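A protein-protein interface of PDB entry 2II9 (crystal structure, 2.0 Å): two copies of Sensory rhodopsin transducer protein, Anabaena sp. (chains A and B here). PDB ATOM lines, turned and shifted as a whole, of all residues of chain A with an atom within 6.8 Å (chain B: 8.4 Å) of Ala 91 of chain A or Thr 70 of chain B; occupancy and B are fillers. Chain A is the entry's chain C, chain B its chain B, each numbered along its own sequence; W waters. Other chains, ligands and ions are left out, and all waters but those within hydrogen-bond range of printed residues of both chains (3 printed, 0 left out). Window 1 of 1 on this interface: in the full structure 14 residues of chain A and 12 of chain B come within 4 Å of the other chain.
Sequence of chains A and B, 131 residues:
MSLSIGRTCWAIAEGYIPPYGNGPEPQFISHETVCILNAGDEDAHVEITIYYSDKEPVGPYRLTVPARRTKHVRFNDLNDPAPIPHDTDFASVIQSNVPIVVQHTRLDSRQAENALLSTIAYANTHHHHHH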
ATOM      1  N   ILE A  12     -19.927 -25.836 -20.843  1.00  0.00           N
ATOM      2  CA  ILE A  12     -18.685 -26.407 -20.289  1.00  0.00           C
ATOM      3  C   ILE A  12     -17.482 -25.842 -21.072  1.00  0.00           C
ATOM      4  O   ILE A  12     -17.333 -26.154 -22.228  1.00  0.00           O
ATOM      5  CB  ILE A  12     -18.688 -27.949 -20.410  1.00  0.00           C
ATOM      6  CG1 ILE A  12     -19.866 -28.542 -19.651  1.00  0.00           C
ATOM      7  CG2 ILE A  12     -17.366 -28.580 -19.960  1.00  0.00           C
ATOM      8  CD1 ILE A  12     -20.159 -29.926 -20.069  1.00  0.00           C
ATOM      9  N   ALA A  13     -16.646 -25.016 -20.419  1.00  0.00           N
ATOM     10  CA  ALA A  13     -15.538 -24.288 -21.045  1.00  0.00           C
ATOM     11  C   ALA A  13     -14.310 -25.160 -21.356  1.00  0.00           C
ATOM     12  O   ALA A  13     -13.452 -24.727 -22.133  1.00  0.00           O
ATOM     13  CB  ALA A  13     -15.119 -23.073 -20.193  1.00  0.00           C
ATOM     14  N   GLU A  14     -14.240 -26.363 -20.773  1.00  0.00           N
ATOM     15  CA  GLU A  14     -13.158 -27.333 -21.018  1.00  0.00           C
ATOM     16  C   GLU A  14     -13.606 -28.536 -21.871  1.00  0.00           C
ATOM     17  O   GLU A  14     -14.796 -28.843 -21.995  1.00  0.00           O
ATOM     18  CB  GLU A  14     -12.544 -27.830 -19.706  1.00  0.00           C
ATOM     19  CG  GLU A  14     -11.396 -28.899 -19.875  1.00  0.00           C
ATOM     20  CD  GLU A  14     -10.094 -28.372 -20.555  1.00  0.00           C
ATOM     21  OE1 GLU A  14      -9.877 -28.597 -21.779  1.00  0.00           O
ATOM     22  OE2 GLU A  14      -9.259 -27.742 -19.851  1.00  0.00           O
ATOM     23  N   GLY A  15     -12.647 -29.212 -22.465  1.00  0.00           N
ATOM     24  CA  GLY A  15     -12.936 -30.351 -23.289  1.00  0.00           C
ATOM     25  C   GLY A  15     -11.638 -30.773 -23.886  1.00  0.00           C
ATOM     26  O   GLY A  15     -10.931 -29.950 -24.440  1.00  0.00           O
ATOM     27  N   ILE A  48     -26.021 -30.551 -28.495  1.00  0.00           N
ATOM     28  CA  ILE A  48     -24.700 -30.140 -28.054  1.00  0.00           C
ATOM     29  C   ILE A  48     -23.966 -29.455 -29.229  1.00  0.00           C
ATOM     30  O   ILE A  48     -24.021 -29.935 -30.364  1.00  0.00           O
ATOM     31  CB  ILE A  48     -23.915 -31.336 -27.540  1.00  0.00           C
ATOM     32  CG1 ILE A  48     -24.591 -31.907 -26.280  1.00  0.00           C
ATOM     33  CG2 ILE A  48     -22.429 -30.990 -27.334  1.00  0.00           C
ATOM     34  CD1 ILE A  48     -24.103 -33.291 -25.879  1.00  0.00           C
ATOM     35  N   THR A  49     -23.429 -28.269 -28.962  1.00  0.00           N
ATOM     36  CA  THR A  49     -22.575 -27.536 -29.937  1.00  0.00           C
ATOM     37  C   THR A  49     -21.183 -27.544 -29.343  1.00  0.00           C
ATOM     38  O   THR A  49     -21.034 -27.264 -28.165  1.00  0.00           O
ATOM     39  CB  THR A  49     -23.027 -26.084 -30.126  1.00  0.00           C
ATOM     40  OG1 THR A  49     -24.382 -26.079 -30.603  1.00  0.00           O
ATOM     41  CG2 THR A  49     -22.143 -25.356 -31.165  1.00  0.00           C
ATOM     42  N   ILE A  50     -20.203 -27.823 -30.184  1.00  0.00           N
ATOM     43  CA  ILE A  50     -18.813 -27.878 -29.828  1.00  0.00           C
ATOM     44  C   ILE A  50     -18.052 -26.697 -30.425  1.00  0.00           C
ATOM     45  O   ILE A  50     -18.173 -26.429 -31.627  1.00  0.00           O
ATOM     46  CB  ILE A  50     -18.139 -29.191 -30.290  1.00  0.00           C
ATOM     47  CG1 ILE A  50     -18.931 -30.424 -29.775  1.00  0.00           C
ATOM     48  CG2 ILE A  50     -16.561 -29.212 -29.976  1.00  0.00           C
ATOM     49  CD1 ILE A  50     -18.838 -30.731 -28.284  1.00  0.00           C
ATOM     50  N   TYR A  51     -17.291 -26.016 -29.564  1.00  0.00           N
ATOM     51  CA  TYR A  51     -16.543 -24.813 -29.895  1.00  0.00           C
ATOM     52  C   TYR A  51     -15.075 -25.126 -29.850  1.00  0.00           C
ATOM     53  O   TYR A  51     -14.627 -26.042 -29.113  1.00  0.00           O
ATOM     54  CB  TYR A  51     -16.855 -23.657 -28.923  1.00  0.00           C
ATOM     55  CG  TYR A  51     -18.278 -23.133 -29.046  1.00  0.00           C
ATOM     56  CD1 TYR A  51     -18.547 -21.938 -29.773  1.00  0.00           C
ATOM     57  CD2 TYR A  51     -19.345 -23.801 -28.422  1.00  0.00           C
ATOM     58  CE1 TYR A  51     -19.819 -21.465 -29.926  1.00  0.00           C
ATOM     59  CE2 TYR A  51     -20.660 -23.314 -28.565  1.00  0.00           C
ATOM     60  CZ  TYR A  51     -20.870 -22.175 -29.305  1.00  0.00           C
ATOM     61  OH  TYR A  51     -22.108 -21.720 -29.441  1.00  0.00           O
ATOM     62  N   TYR A  52     -14.330 -24.372 -30.648  1.00  0.00           N
ATOM     63  CA  TYR A  52     -12.912 -24.568 -30.869  1.00  0.00           C
ATOM     64  C   TYR A  52     -12.172 -23.273 -30.742  1.00  0.00           C
ATOM     65  O   TYR A  52     -12.781 -22.207 -30.765  1.00  0.00           O
ATOM     66  CB  TYR A  52     -12.684 -25.119 -32.302  1.00  0.00           C
ATOM     67  CG  TYR A  52     -13.186 -26.524 -32.423  1.00  0.00           C
ATOM     68  CD1 TYR A  52     -12.508 -27.571 -31.809  1.00  0.00           C
ATOM     69  CD2 TYR A  52     -14.415 -26.795 -33.056  1.00  0.00           C
ATOM     70  CE1 TYR A  52     -13.013 -28.879 -31.855  1.00  0.00           C
ATOM     71  CE2 TYR A  52     -14.900 -28.087 -33.128  1.00  0.00           C
ATOM     72  CZ  TYR A  52     -14.207 -29.127 -32.516  1.00  0.00           C
ATOM     73  OH  TYR A  52     -14.712 -30.443 -32.576  1.00  0.00           O
ATOM     74  N   SER A  53     -10.840 -23.345 -30.681  1.00  0.00           N
ATOM     75  CA  SER A  53     -10.076 -22.128 -30.530  1.00  0.00           C
ATOM     76  C   SER A  53      -9.807 -21.426 -31.884  1.00  0.00           C
ATOM     77  O   SER A  53      -9.510 -20.250 -31.945  1.00  0.00           O
ATOM     78  CB  SER A  53      -8.780 -22.455 -29.837  1.00  0.00           C
ATOM     79  OG  SER A  53      -8.004 -23.207 -30.724  1.00  0.00           O
ATOM     80  N   ASP A  54      -9.942 -22.150 -32.978  1.00  0.00           N
ATOM     81  CA  ASP A  54      -9.461 -21.609 -34.222  1.00  0.00           C
ATOM     82  C   ASP A  54     -10.377 -21.895 -35.428  1.00  0.00           C
ATOM     83  O   ASP A  54      -9.909 -21.803 -36.566  1.00  0.00           O
ATOM     84  CB  ASP A  54      -8.082 -22.204 -34.485  1.00  0.00           C
ATOM     85  CG  ASP A  54      -8.123 -23.738 -34.578  1.00  0.00           C
ATOM     86  OD1 ASP A  54      -9.206 -24.348 -34.457  1.00  0.00           O
ATOM     87  OD2 ASP A  54      -7.060 -24.340 -34.796  1.00  0.00           O
ATOM     88  N   LYS A  55     -11.652 -22.222 -35.187  1.00  0.00           N
ATOM     89  CA  LYS A  55     -12.591 -22.559 -36.274  1.00  0.00           C
ATOM     90  C   LYS A  55     -14.023 -22.477 -35.779  1.00  0.00           C
ATOM     91  O   LYS A  55     -14.215 -22.449 -34.573  1.00  0.00           O
ATOM     92  CB  LYS A  55     -12.292 -23.964 -36.812  1.00  0.00           C
ATOM     93  CG  LYS A  55     -12.561 -25.139 -35.893  1.00  0.00           C
ATOM     94  CD  LYS A  55     -12.492 -26.433 -36.703  1.00  0.00           C
ATOM     95  CE  LYS A  55     -12.067 -27.601 -35.878  1.00  0.00           C
ATOM     96  NZ  LYS A  55     -11.958 -28.909 -36.642  1.00  0.00           N
ATOM     97  N   PHE A  75     -17.739 -37.771 -25.070  1.00  0.00           N
ATOM     98  CA  PHE A  75     -17.471 -36.840 -26.180  1.00  0.00           C
ATOM     99  C   PHE A  75     -16.785 -37.577 -27.333  1.00  0.00           C
ATOM    100  O   PHE A  75     -16.957 -37.271 -28.514  1.00  0.00           O
ATOM    101  CB  PHE A  75     -16.602 -35.691 -25.720  1.00  0.00           C
ATOM    102  CG  PHE A  75     -17.372 -34.569 -25.057  1.00  0.00           C
ATOM    103  CD1 PHE A  75     -18.390 -33.895 -25.728  1.00  0.00           C
ATOM    104  CD2 PHE A  75     -17.032 -34.158 -23.767  1.00  0.00           C
ATOM    105  CE1 PHE A  75     -19.099 -32.845 -25.116  1.00  0.00           C
ATOM    106  CE2 PHE A  75     -17.724 -33.100 -23.137  1.00  0.00           C
ATOM    107  CZ  PHE A  75     -18.773 -32.461 -23.819  1.00  0.00           C
ATOM    108  N   ASP A  89      -8.249 -28.780 -27.820  1.00  0.00           N
ATOM    109  CA  ASP A  89      -9.062 -28.129 -26.784  1.00  0.00           C
ATOM    110  C   ASP A  89     -10.389 -27.672 -27.385  1.00  0.00           C
ATOM    111  O   ASP A  89     -10.427 -27.105 -28.479  1.00  0.00           O
ATOM    112  CB  ASP A  89      -8.372 -26.892 -26.200  1.00  0.00           C
ATOM    113  CG  ASP A  89      -7.060 -27.220 -25.533  1.00  0.00           C
ATOM    114  OD1 ASP A  89      -6.853 -28.355 -25.024  1.00  0.00           O
ATOM    115  OD2 ASP A  89      -6.253 -26.290 -25.503  1.00  0.00           O
ATOM    116  N   PHE A  90     -11.456 -27.896 -26.654  1.00  0.00           N
ATOM    117  CA  PHE A  90     -12.798 -27.528 -27.130  1.00  0.00           C
ATOM    118  C   PHE A  90     -13.688 -27.168 -25.933  1.00  0.00           C
ATOM    119  O   PHE A  90     -13.278 -27.278 -24.796  1.00  0.00           O
ATOM    120  CB  PHE A  90     -13.427 -28.636 -27.999  1.00  0.00           C
ATOM    121  CG  PHE A  90     -13.709 -29.929 -27.268  1.00  0.00           C
ATOM    122  CD1 PHE A  90     -14.946 -30.154 -26.676  1.00  0.00           C
ATOM    123  CD2 PHE A  90     -12.761 -30.966 -27.247  1.00  0.00           C
ATOM    124  CE1 PHE A  90     -15.230 -31.335 -26.047  1.00  0.00           C
ATOM    125  CE2 PHE A  90     -13.017 -32.139 -26.584  1.00  0.00           C
ATOM    126  CZ  PHE A  90     -14.279 -32.332 -25.985  1.00  0.00           C
ATOM    127  N   ALA A  91     -14.909 -26.773 -26.206  1.00  0.00           N
ATOM    128  CA  ALA A  91     -15.817 -26.321 -25.193  1.00  0.00           C
ATOM    129  C   ALA A  91     -17.174 -26.748 -25.736  1.00  0.00           C
ATOM    130  O   ALA A  91     -17.304 -26.985 -26.930  1.00  0.00           O
ATOM    131  CB  ALA A  91     -15.719 -24.841 -25.042  1.00  0.00           C
ATOM    132  N   SER A  92     -18.160 -26.956 -24.882  1.00  0.00           N
ATOM    133  CA  SER A  92     -19.483 -27.358 -25.394  1.00  0.00           C
ATOM    134  C   SER A  92     -20.576 -26.465 -24.770  1.00  0.00           C
ATOM    135  O   SER A  92     -20.379 -25.881 -23.671  1.00  0.00           O
ATOM    136  CB  SER A  92     -19.714 -28.851 -25.151  1.00  0.00           C
ATOM    137  OG  SER A  92     -19.693 -29.173 -23.770  1.00  0.00           O
ATOM    138  N   VAL A  93     -21.649 -26.252 -25.523  1.00  0.00           N
ATOM    139  CA  VAL A  93     -22.896 -25.760 -24.996  1.00  0.00           C
ATOM    140  C   VAL A  93     -23.952 -26.904 -25.155  1.00  0.00           C
ATOM    141  O   VAL A  93     -24.053 -27.551 -26.207  1.00  0.00           O
ATOM    142  CB  VAL A  93     -23.338 -24.565 -25.804  1.00  0.00           C
ATOM    143  CG1 VAL A  93     -24.795 -24.152 -25.409  1.00  0.00           C
ATOM    144  CG2 VAL A  93     -22.377 -23.410 -25.590  1.00  0.00           C
ATOM    145  N   VAL B  34      -6.679 -21.385 -17.346  1.00  0.00           N
ATOM    146  CA  VAL B  34      -8.086 -20.916 -17.318  1.00  0.00           C
ATOM    147  C   VAL B  34      -8.635 -21.123 -18.714  1.00  0.00           C
ATOM    148  O   VAL B  34      -7.963 -20.752 -19.667  1.00  0.00           O
ATOM    149  CB  VAL B  34      -8.165 -19.459 -16.870  1.00  0.00           C
ATOM    150  CG1 VAL B  34      -9.514 -18.816 -17.189  1.00  0.00           C
ATOM    151  CG2 VAL B  34      -7.893 -19.400 -15.380  1.00  0.00           C
ATOM    152  N   CYS B  35      -9.807 -21.753 -18.824  1.00  0.00           N
ATOM    153  CA  CYS B  35     -10.466 -21.985 -20.109  1.00  0.00           C
ATOM    154  C   CYS B  35     -11.663 -21.101 -20.249  1.00  0.00           C
ATOM    155  O   CYS B  35     -12.520 -21.066 -19.342  1.00  0.00           O
ATOM    156  CB  CYS B  35     -10.929 -23.440 -20.240  1.00  0.00           C
ATOM    157  SG  CYS B  35      -9.550 -24.610 -20.082  1.00  0.00           S
ATOM    158  N   ILE B  36     -11.719 -20.362 -21.375  1.00  0.00           N
ATOM    159  CA  ILE B  36     -12.727 -19.324 -21.545  1.00  0.00           C
ATOM    160  C   ILE B  36     -13.533 -19.656 -22.789  1.00  0.00           C
ATOM    161  O   ILE B  36     -12.965 -19.847 -23.829  1.00  0.00           O
ATOM    162  CB  ILE B  36     -12.099 -17.902 -21.726  1.00  0.00           C
ATOM    163  CG1 ILE B  36     -11.179 -17.524 -20.521  1.00  0.00           C
ATOM    164  CG2 ILE B  36     -13.193 -16.859 -21.960  1.00  0.00           C
ATOM    165  CD1 ILE B  36     -10.482 -16.163 -20.619  1.00  0.00           C
ATOM    166  N   LEU B  37     -14.843 -19.687 -22.680  1.00  0.00           N
ATOM    167  CA  LEU B  37     -15.681 -19.838 -23.847  1.00  0.00           C
ATOM    168  C   LEU B  37     -16.375 -18.513 -24.168  1.00  0.00           C
ATOM    169  O   LEU B  37     -17.027 -17.926 -23.338  1.00  0.00           O
ATOM    170  CB  LEU B  37     -16.723 -20.936 -23.608  1.00  0.00           C
ATOM    171  CG  LEU B  37     -17.935 -21.065 -24.534  1.00  0.00           C
ATOM    172  CD1 LEU B  37     -17.455 -21.274 -26.005  1.00  0.00           C
ATOM    173  CD2 LEU B  37     -18.790 -22.200 -24.055  1.00  0.00           C
ATOM    174  N   ASN B  38     -16.228 -18.036 -25.393  1.00  0.00           N
ATOM    175  CA  ASN B  38     -17.107 -16.993 -25.868  1.00  0.00           C
ATOM    176  C   ASN B  38     -18.094 -17.598 -26.924  1.00  0.00           C
ATOM    177  O   ASN B  38     -17.728 -17.728 -28.099  1.00  0.00           O
ATOM    178  CB  ASN B  38     -16.304 -15.845 -26.475  1.00  0.00           C
ATOM    179  CG  ASN B  38     -17.187 -14.750 -27.026  1.00  0.00           C
ATOM    180  OD1 ASN B  38     -18.405 -14.724 -26.813  1.00  0.00           O
ATOM    181  ND2 ASN B  38     -16.582 -13.820 -27.691  1.00  0.00           N
ATOM    182  N   ALA B  39     -19.301 -18.000 -26.481  1.00  0.00           N
ATOM    183  CA  ALA B  39     -20.315 -18.583 -27.388  1.00  0.00           C
ATOM    184  C   ALA B  39     -21.097 -17.529 -28.165  1.00  0.00           C
ATOM    185  O   ALA B  39     -21.986 -17.879 -28.969  1.00  0.00           O
ATOM    186  CB  ALA B  39     -21.291 -19.460 -26.637  1.00  0.00           C
ATOM    187  N   THR B  64      -8.030 -11.402 -26.074  1.00  0.00           N
ATOM    188  CA  THR B  64      -9.297 -11.408 -26.802  1.00  0.00           C
ATOM    189  C   THR B  64      -9.718 -12.821 -26.983  1.00  0.00           C
ATOM    190  O   THR B  64      -8.915 -13.678 -27.350  1.00  0.00           O
ATOM    191  CB  THR B  64      -9.208 -10.691 -28.170  1.00  0.00           C
ATOM    192  OG1 THR B  64      -8.887  -9.312 -27.973  1.00  0.00           O
ATOM    193  CG2 THR B  64     -10.552 -10.771 -28.976  1.00  0.00           C
ATOM    194  N   VAL B  65     -10.984 -13.110 -26.703  1.00  0.00           N
ATOM    195  CA  VAL B  65     -11.513 -14.437 -27.066  1.00  0.00           C
ATOM    196  C   VAL B  65     -12.518 -14.145 -28.191  1.00  0.00           C
ATOM    197  O   VAL B  65     -13.596 -13.531 -27.911  1.00  0.00           O
ATOM    198  CB  VAL B  65     -12.205 -15.097 -25.874  1.00  0.00           C
ATOM    199  CG1 VAL B  65     -12.718 -16.531 -26.243  1.00  0.00           C
ATOM    200  CG2 VAL B  65     -11.193 -15.118 -24.658  1.00  0.00           C
ATOM    201  N   PRO B  66     -12.161 -14.500 -29.454  1.00  0.00           N
ATOM    202  CA  PRO B  66     -13.052 -14.091 -30.552  1.00  0.00           C
ATOM    203  C   PRO B  66     -14.445 -14.708 -30.428  1.00  0.00           C
ATOM    204  O   PRO B  66     -14.606 -15.697 -29.717  1.00  0.00           O
ATOM    205  CB  PRO B  66     -12.330 -14.649 -31.797  1.00  0.00           C
ATOM    206  CG  PRO B  66     -10.869 -14.639 -31.431  1.00  0.00           C
ATOM    207  CD  PRO B  66     -10.966 -15.174 -29.975  1.00  0.00           C
ATOM    208  N   ALA B  67     -15.408 -14.146 -31.157  1.00  0.00           N
ATOM    209  CA  ALA B  67     -16.780 -14.631 -31.306  1.00  0.00           C
ATOM    210  C   ALA B  67     -16.763 -16.133 -31.603  1.00  0.00           C
ATOM    211  O   ALA B  67     -16.004 -16.584 -32.426  1.00  0.00           O
ATOM    212  CB  ALA B  67     -17.426 -13.881 -32.443  1.00  0.00           C
ATOM    213  N   ARG B  68     -17.581 -16.911 -30.886  1.00  0.00           N
ATOM    214  CA  ARG B  68     -17.747 -18.368 -31.132  1.00  0.00           C
ATOM    215  C   ARG B  68     -16.441 -19.153 -31.090  1.00  0.00           C
ATOM    216  O   ARG B  68     -16.178 -20.037 -31.940  1.00  0.00           O
ATOM    217  CB  ARG B  68     -18.474 -18.567 -32.489  1.00  0.00           C
ATOM    218  CG  ARG B  68     -19.861 -17.885 -32.557  1.00  0.00           C
ATOM    219  CD  ARG B  68     -20.494 -18.016 -33.956  1.00  0.00           C
ATOM    220  NE  ARG B  68     -19.553 -17.527 -34.954  1.00  0.00           N
ATOM    221  CZ  ARG B  68     -19.347 -16.249 -35.207  1.00  0.00           C
ATOM    222  NH1 ARG B  68     -20.073 -15.339 -34.593  1.00  0.00           N
ATOM    223  NH2 ARG B  68     -18.434 -15.886 -36.096  1.00  0.00           N
ATOM    224  N   ARG B  69     -15.611 -18.859 -30.086  1.00  0.00           N
ATOM    225  CA  ARG B  69     -14.353 -19.501 -29.889  1.00  0.00           C
ATOM    226  C   ARG B  69     -14.125 -19.759 -28.412  1.00  0.00           C
ATOM    227  O   ARG B  69     -14.632 -19.026 -27.537  1.00  0.00           O
ATOM    228  CB  ARG B  69     -13.181 -18.654 -30.401  1.00  0.00           C
ATOM    229  CG  ARG B  69     -13.121 -18.405 -31.947  1.00  0.00           C
ATOM    230  CD  ARG B  69     -13.114 -19.641 -32.827  1.00  0.00           C
ATOM    231  NE  ARG B  69     -12.983 -19.273 -34.251  1.00  0.00           N
ATOM    232  CZ  ARG B  69     -14.011 -19.070 -35.068  1.00  0.00           C
ATOM    233  NH1 ARG B  69     -15.287 -19.147 -34.601  1.00  0.00           N
ATOM    234  NH2 ARG B  69     -13.773 -18.720 -36.317  1.00  0.00           N
ATOM    235  N   THR B  70     -13.329 -20.793 -28.155  1.00  0.00           N
ATOM    236  CA  THR B  70     -12.791 -21.022 -26.843  1.00  0.00           C
ATOM    237  C   THR B  70     -11.310 -20.663 -26.834  1.00  0.00           C
ATOM    238  O   THR B  70     -10.680 -20.687 -27.869  1.00  0.00           O
ATOM    239  CB  THR B  70     -13.125 -22.464 -26.284  1.00  0.00           C
ATOM    240  OG1 THR B  70     -12.599 -22.549 -24.946  1.00  0.00           O
ATOM    241  CG2 THR B  70     -12.546 -23.525 -27.087  1.00  0.00           C
ATOM    242  N   LYS B  71     -10.772 -20.256 -25.680  1.00  0.00           N
ATOM    243  CA  LYS B  71      -9.346 -20.026 -25.535  1.00  0.00           C
ATOM    244  C   LYS B  71      -8.865 -20.581 -24.199  1.00  0.00           C
ATOM    245  O   LYS B  71      -9.491 -20.370 -23.165  1.00  0.00           O
ATOM    246  CB  LYS B  71      -9.010 -18.533 -25.625  1.00  0.00           C
ATOM    247  CG  LYS B  71      -7.514 -18.200 -25.918  1.00  0.00           C
ATOM    248  CD  LYS B  71      -7.188 -16.711 -25.600  1.00  0.00           C
ATOM    249  CE  LYS B  71      -5.922 -16.160 -26.301  1.00  0.00           C
ATOM    250  NZ  LYS B  71      -6.378 -15.200 -27.415  1.00  0.00           N
ATOM    251  N   HIS B  72      -7.725 -21.253 -24.243  1.00  0.00           N
ATOM    252  CA  HIS B  72      -7.015 -21.741 -23.038  1.00  0.00           C
ATOM    253  C   HIS B  72      -5.922 -20.802 -22.664  1.00  0.00           C
ATOM    254  O   HIS B  72      -5.060 -20.460 -23.475  1.00  0.00           O
ATOM    255  CB  HIS B  72      -6.365 -23.068 -23.310  1.00  0.00           C
ATOM    256  CG  HIS B  72      -7.251 -24.220 -23.005  1.00  0.00           C
ATOM    257  ND1 HIS B  72      -6.774 -25.398 -22.458  1.00  0.00           N
ATOM    258  CD2 HIS B  72      -8.594 -24.374 -23.155  1.00  0.00           C
ATOM    259  CE1 HIS B  72      -7.789 -26.235 -22.302  1.00  0.00           C
ATOM    260  NE2 HIS B  72      -8.906 -25.635 -22.709  1.00  0.00           N
ATOM    261  N   VAL B  73      -5.982 -20.323 -21.443  1.00  0.00           N
ATOM    262  CA  VAL B  73      -5.049 -19.321 -21.013  1.00  0.00           C
ATOM    263  C   VAL B  73      -4.125 -19.953 -19.938  1.00  0.00           C
ATOM    264  O   VAL B  73      -4.580 -20.374 -18.865  1.00  0.00           O
ATOM    265  CB  VAL B  73      -5.775 -18.039 -20.520  1.00  0.00           C
ATOM    266  CG1 VAL B  73      -4.740 -16.956 -20.138  1.00  0.00           C
ATOM    267  CG2 VAL B  73      -6.690 -17.448 -21.647  1.00  0.00           C
ATOM    268  N   VAL B 101     -17.876 -17.795 -20.532  1.00  0.00           N
ATOM    269  CA  VAL B 101     -17.889 -18.887 -19.508  1.00  0.00           C
ATOM    270  C   VAL B 101     -16.441 -19.188 -19.218  1.00  0.00           C
ATOM    271  O   VAL B 101     -15.640 -19.288 -20.137  1.00  0.00           O
ATOM    272  CB  VAL B 101     -18.607 -20.107 -20.042  1.00  0.00           C
ATOM    273  CG1 VAL B 101     -18.592 -21.283 -19.050  1.00  0.00           C
ATOM    274  CG2 VAL B 101     -20.050 -19.717 -20.363  1.00  0.00           C
ATOM    275  N   VAL B 102     -16.101 -19.270 -17.926  1.00  0.00           N
ATOM    276  CA  VAL B 102     -14.720 -19.466 -17.482  1.00  0.00           C
ATOM    277  C   VAL B 102     -14.679 -20.689 -16.575  1.00  0.00           C
ATOM    278  O   VAL B 102     -15.502 -20.823 -15.673  1.00  0.00           O
ATOM    279  CB  VAL B 102     -14.154 -18.279 -16.687  1.00  0.00           C
ATOM    280  CG1 VAL B 102     -12.751 -18.604 -16.186  1.00  0.00           C
ATOM    281  CG2 VAL B 102     -14.159 -17.051 -17.489  1.00  0.00           C
ATOM    282  N   GLN B 103     -13.707 -21.534 -16.828  1.00  0.00           N
ATOM    283  CA  GLN B 103     -13.492 -22.694 -15.976  1.00  0.00           C
ATOM    284  C   GLN B 103     -12.007 -22.833 -15.730  1.00  0.00           C
ATOM    285  O   GLN B 103     -11.172 -22.519 -16.572  1.00  0.00           O
ATOM    286  CB  GLN B 103     -14.063 -24.001 -16.567  1.00  0.00           C
ATOM    287  CG  GLN B 103     -13.271 -25.239 -16.043  1.00  0.00           C
ATOM    288  CD  GLN B 103     -13.920 -26.571 -16.300  1.00  0.00           C
ATOM    289  OE1 GLN B 103     -13.230 -27.647 -16.294  1.00  0.00           O
ATOM    290  NE2 GLN B 103     -15.262 -26.543 -16.564  1.00  0.00           N
HETATM  291  O   HOH W   1      -8.745 -18.475 -29.664  1.00  0.00           O
HETATM  292  O   HOH W   2     -15.636 -22.663 -32.459  1.00  0.00           O
HETATM  293  O   HOH W   3     -17.116 -24.814 -17.273  1.00  0.00           O
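Of the 18 printed residues of chain A, 10 touch a printed residue of chain B. Hydrophobic or aromatic side chains of chain A that line the printed part of chain B: Ala 13, Tyr 51 and Ala 91. Of the 19 printed residues of chain B, 9 touch a printed residue of chain A. Hydrophobic or aromatic side chains of chain B within 4 Å of the printed part of chain A: Leu 37, Ala 39 and His 72.
No position is printed for both chains. Of the 20 pairs that touch across the chains among the printed residues, none has its exchanged pair printed and touching as well.
Water W2 lies within hydrogen-bond range of O of Lys 55 of chain A, O of Arg 68 of chain B and N of Tyr 52 of chain A. Water W3 bridges the side-chain amide nitrogen of Gln 103 of chain B (2.6 Å) and the backbone NH of Ala 13 of chain A (3.2 Å). Water W1 lies within hydrogen-bond range of the backbone carbonyl oxygen of Ser 53 of chain A (3.0 Å) and the backbone carbonyl oxygen of Thr 70 of chain B (3.4 Å).
The backbone NH (N) of Arg 68 of chain B lies within hydrogen-bond range of the backbone carbonyl oxygen (O) of Asn 38 of chain B (2.9 Å). The backbone carbonyl oxygen (O) of Val 101 of chain B sits at hydrogen-bond distance from the backbone NH (N) of Leu 37 of chain B, at 2.7 Å. O of Ala 67 of chain B sits at hydrogen-bond distance from NH1 of Arg 69 of chain B, 3.4 Å away. The backbone carbonyl oxygen (O) of Gln 103 of chain B lies within hydrogen-bond range of the backbone NH (N) of Cys 35 of chain B. The backbone NH of Asn 38 of chain B lies within hydrogen-bond range of the backbone carbonyl oxygen of Arg 69 of chain B (2.9 Å). The side-chain hydroxyl of Thr 70 of chain B is in hydrogen-bond range of the backbone carbonyl oxygen of Ile 36 of chain B, at 2.9 Å.
Among the printed residues, pairs that only touch across the chains: Ser 53 of chain A with Thr 70 of chain B (3.1 Å), Tyr 52 of chain A with Arg 69 of chain B (3.2 Å), Ala 13 of chain A with Cys 35 of chain B (3.4 Å), Glu 14 of chain A with Gln 103 of chain B (3.5 Å), Tyr 51 of chain A with Leu 37 of chain B (3.7 Å), Ala 13 of chain A with Thr 70 of chain B (3.7 Å), Tyr 51 of chain A with Ala 39 of chain B (3.7 Å), Ala 91 of chain A with Thr 70 of chain B (3.7 Å), Tyr 51 of chain A with Arg 68 of chain B (3.7 Å), Ser 53 of chain A with Arg 69 of chain B (3.8 Å), Ala 13 of chain A with Val 101 of chain B (3.8 Å), Tyr 51 of chain A with Thr 70 of chain B (3.8 Å), Asp 54 of chain A with Arg 69 of chain B (3.9 Å), Ala 13 of chain A with Gln 103 of chain B (3.9 Å) and Phe 90 of chain A with Thr 70 of chain B (3.99 Å).
Printed residues of chain B within 4 Å of Ser 53 of chain A: Arg 69 and Thr 70. Of the printed residues of chain B, Asp 89 of chain A touches His 72 (3.2 Å). Of the printed residues of chain B, Ala 91 of chain A touches Thr 70. No residue of chain B comes within 4 Å of Ser 92 of chain A. Printed residues of chain A within 4 Å of Thr 70 of chain B: Ala 13 (3.7 Å), Tyr 51 (3.8 Å), Tyr 52 (3.0 Å), Ser 53 (3.1 Å), Phe 90 (3.99 Å) and Ala 91 (3.7 Å). Of the printed residues of chain A, His 72 of chain B touches Glu 14 and Asp 89. Of the printed residues of chain A, Val 101 of chain B touches Ala 13 (3.8 Å). Of the printed residues of chain A, Gln 103 of chain B touches Ala 13 (3.9 Å) and Glu 14 (3.5 Å). The nearest residue of chain B that does not touch Ala 91 of chain A is Leu 37 of chain B (4.1 Å).
A ring nitrogen (ND1) of His 72 of chain B is in hydrogen-bond range of the side-chain carboxylate of Asp 89 of chain A (3.2 Å). The backbone NH of Thr 70 of chain B is in hydrogen-bond range of the backbone carbonyl oxygen of Tyr 52 of chain A. NE2 of His 72 of chain B sits close to OE1 of Glu 14 of chain A (3.3 Å). SG of Cys 35 of chain B sits at hydrogen-bond distance from OE2 of Glu 14 of chain A. The backbone carbonyl oxygen (O) of Lys 55 of chain A lies close to the guanidinium group (NE) of Arg 69 of chain B, at 3.4 Å.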
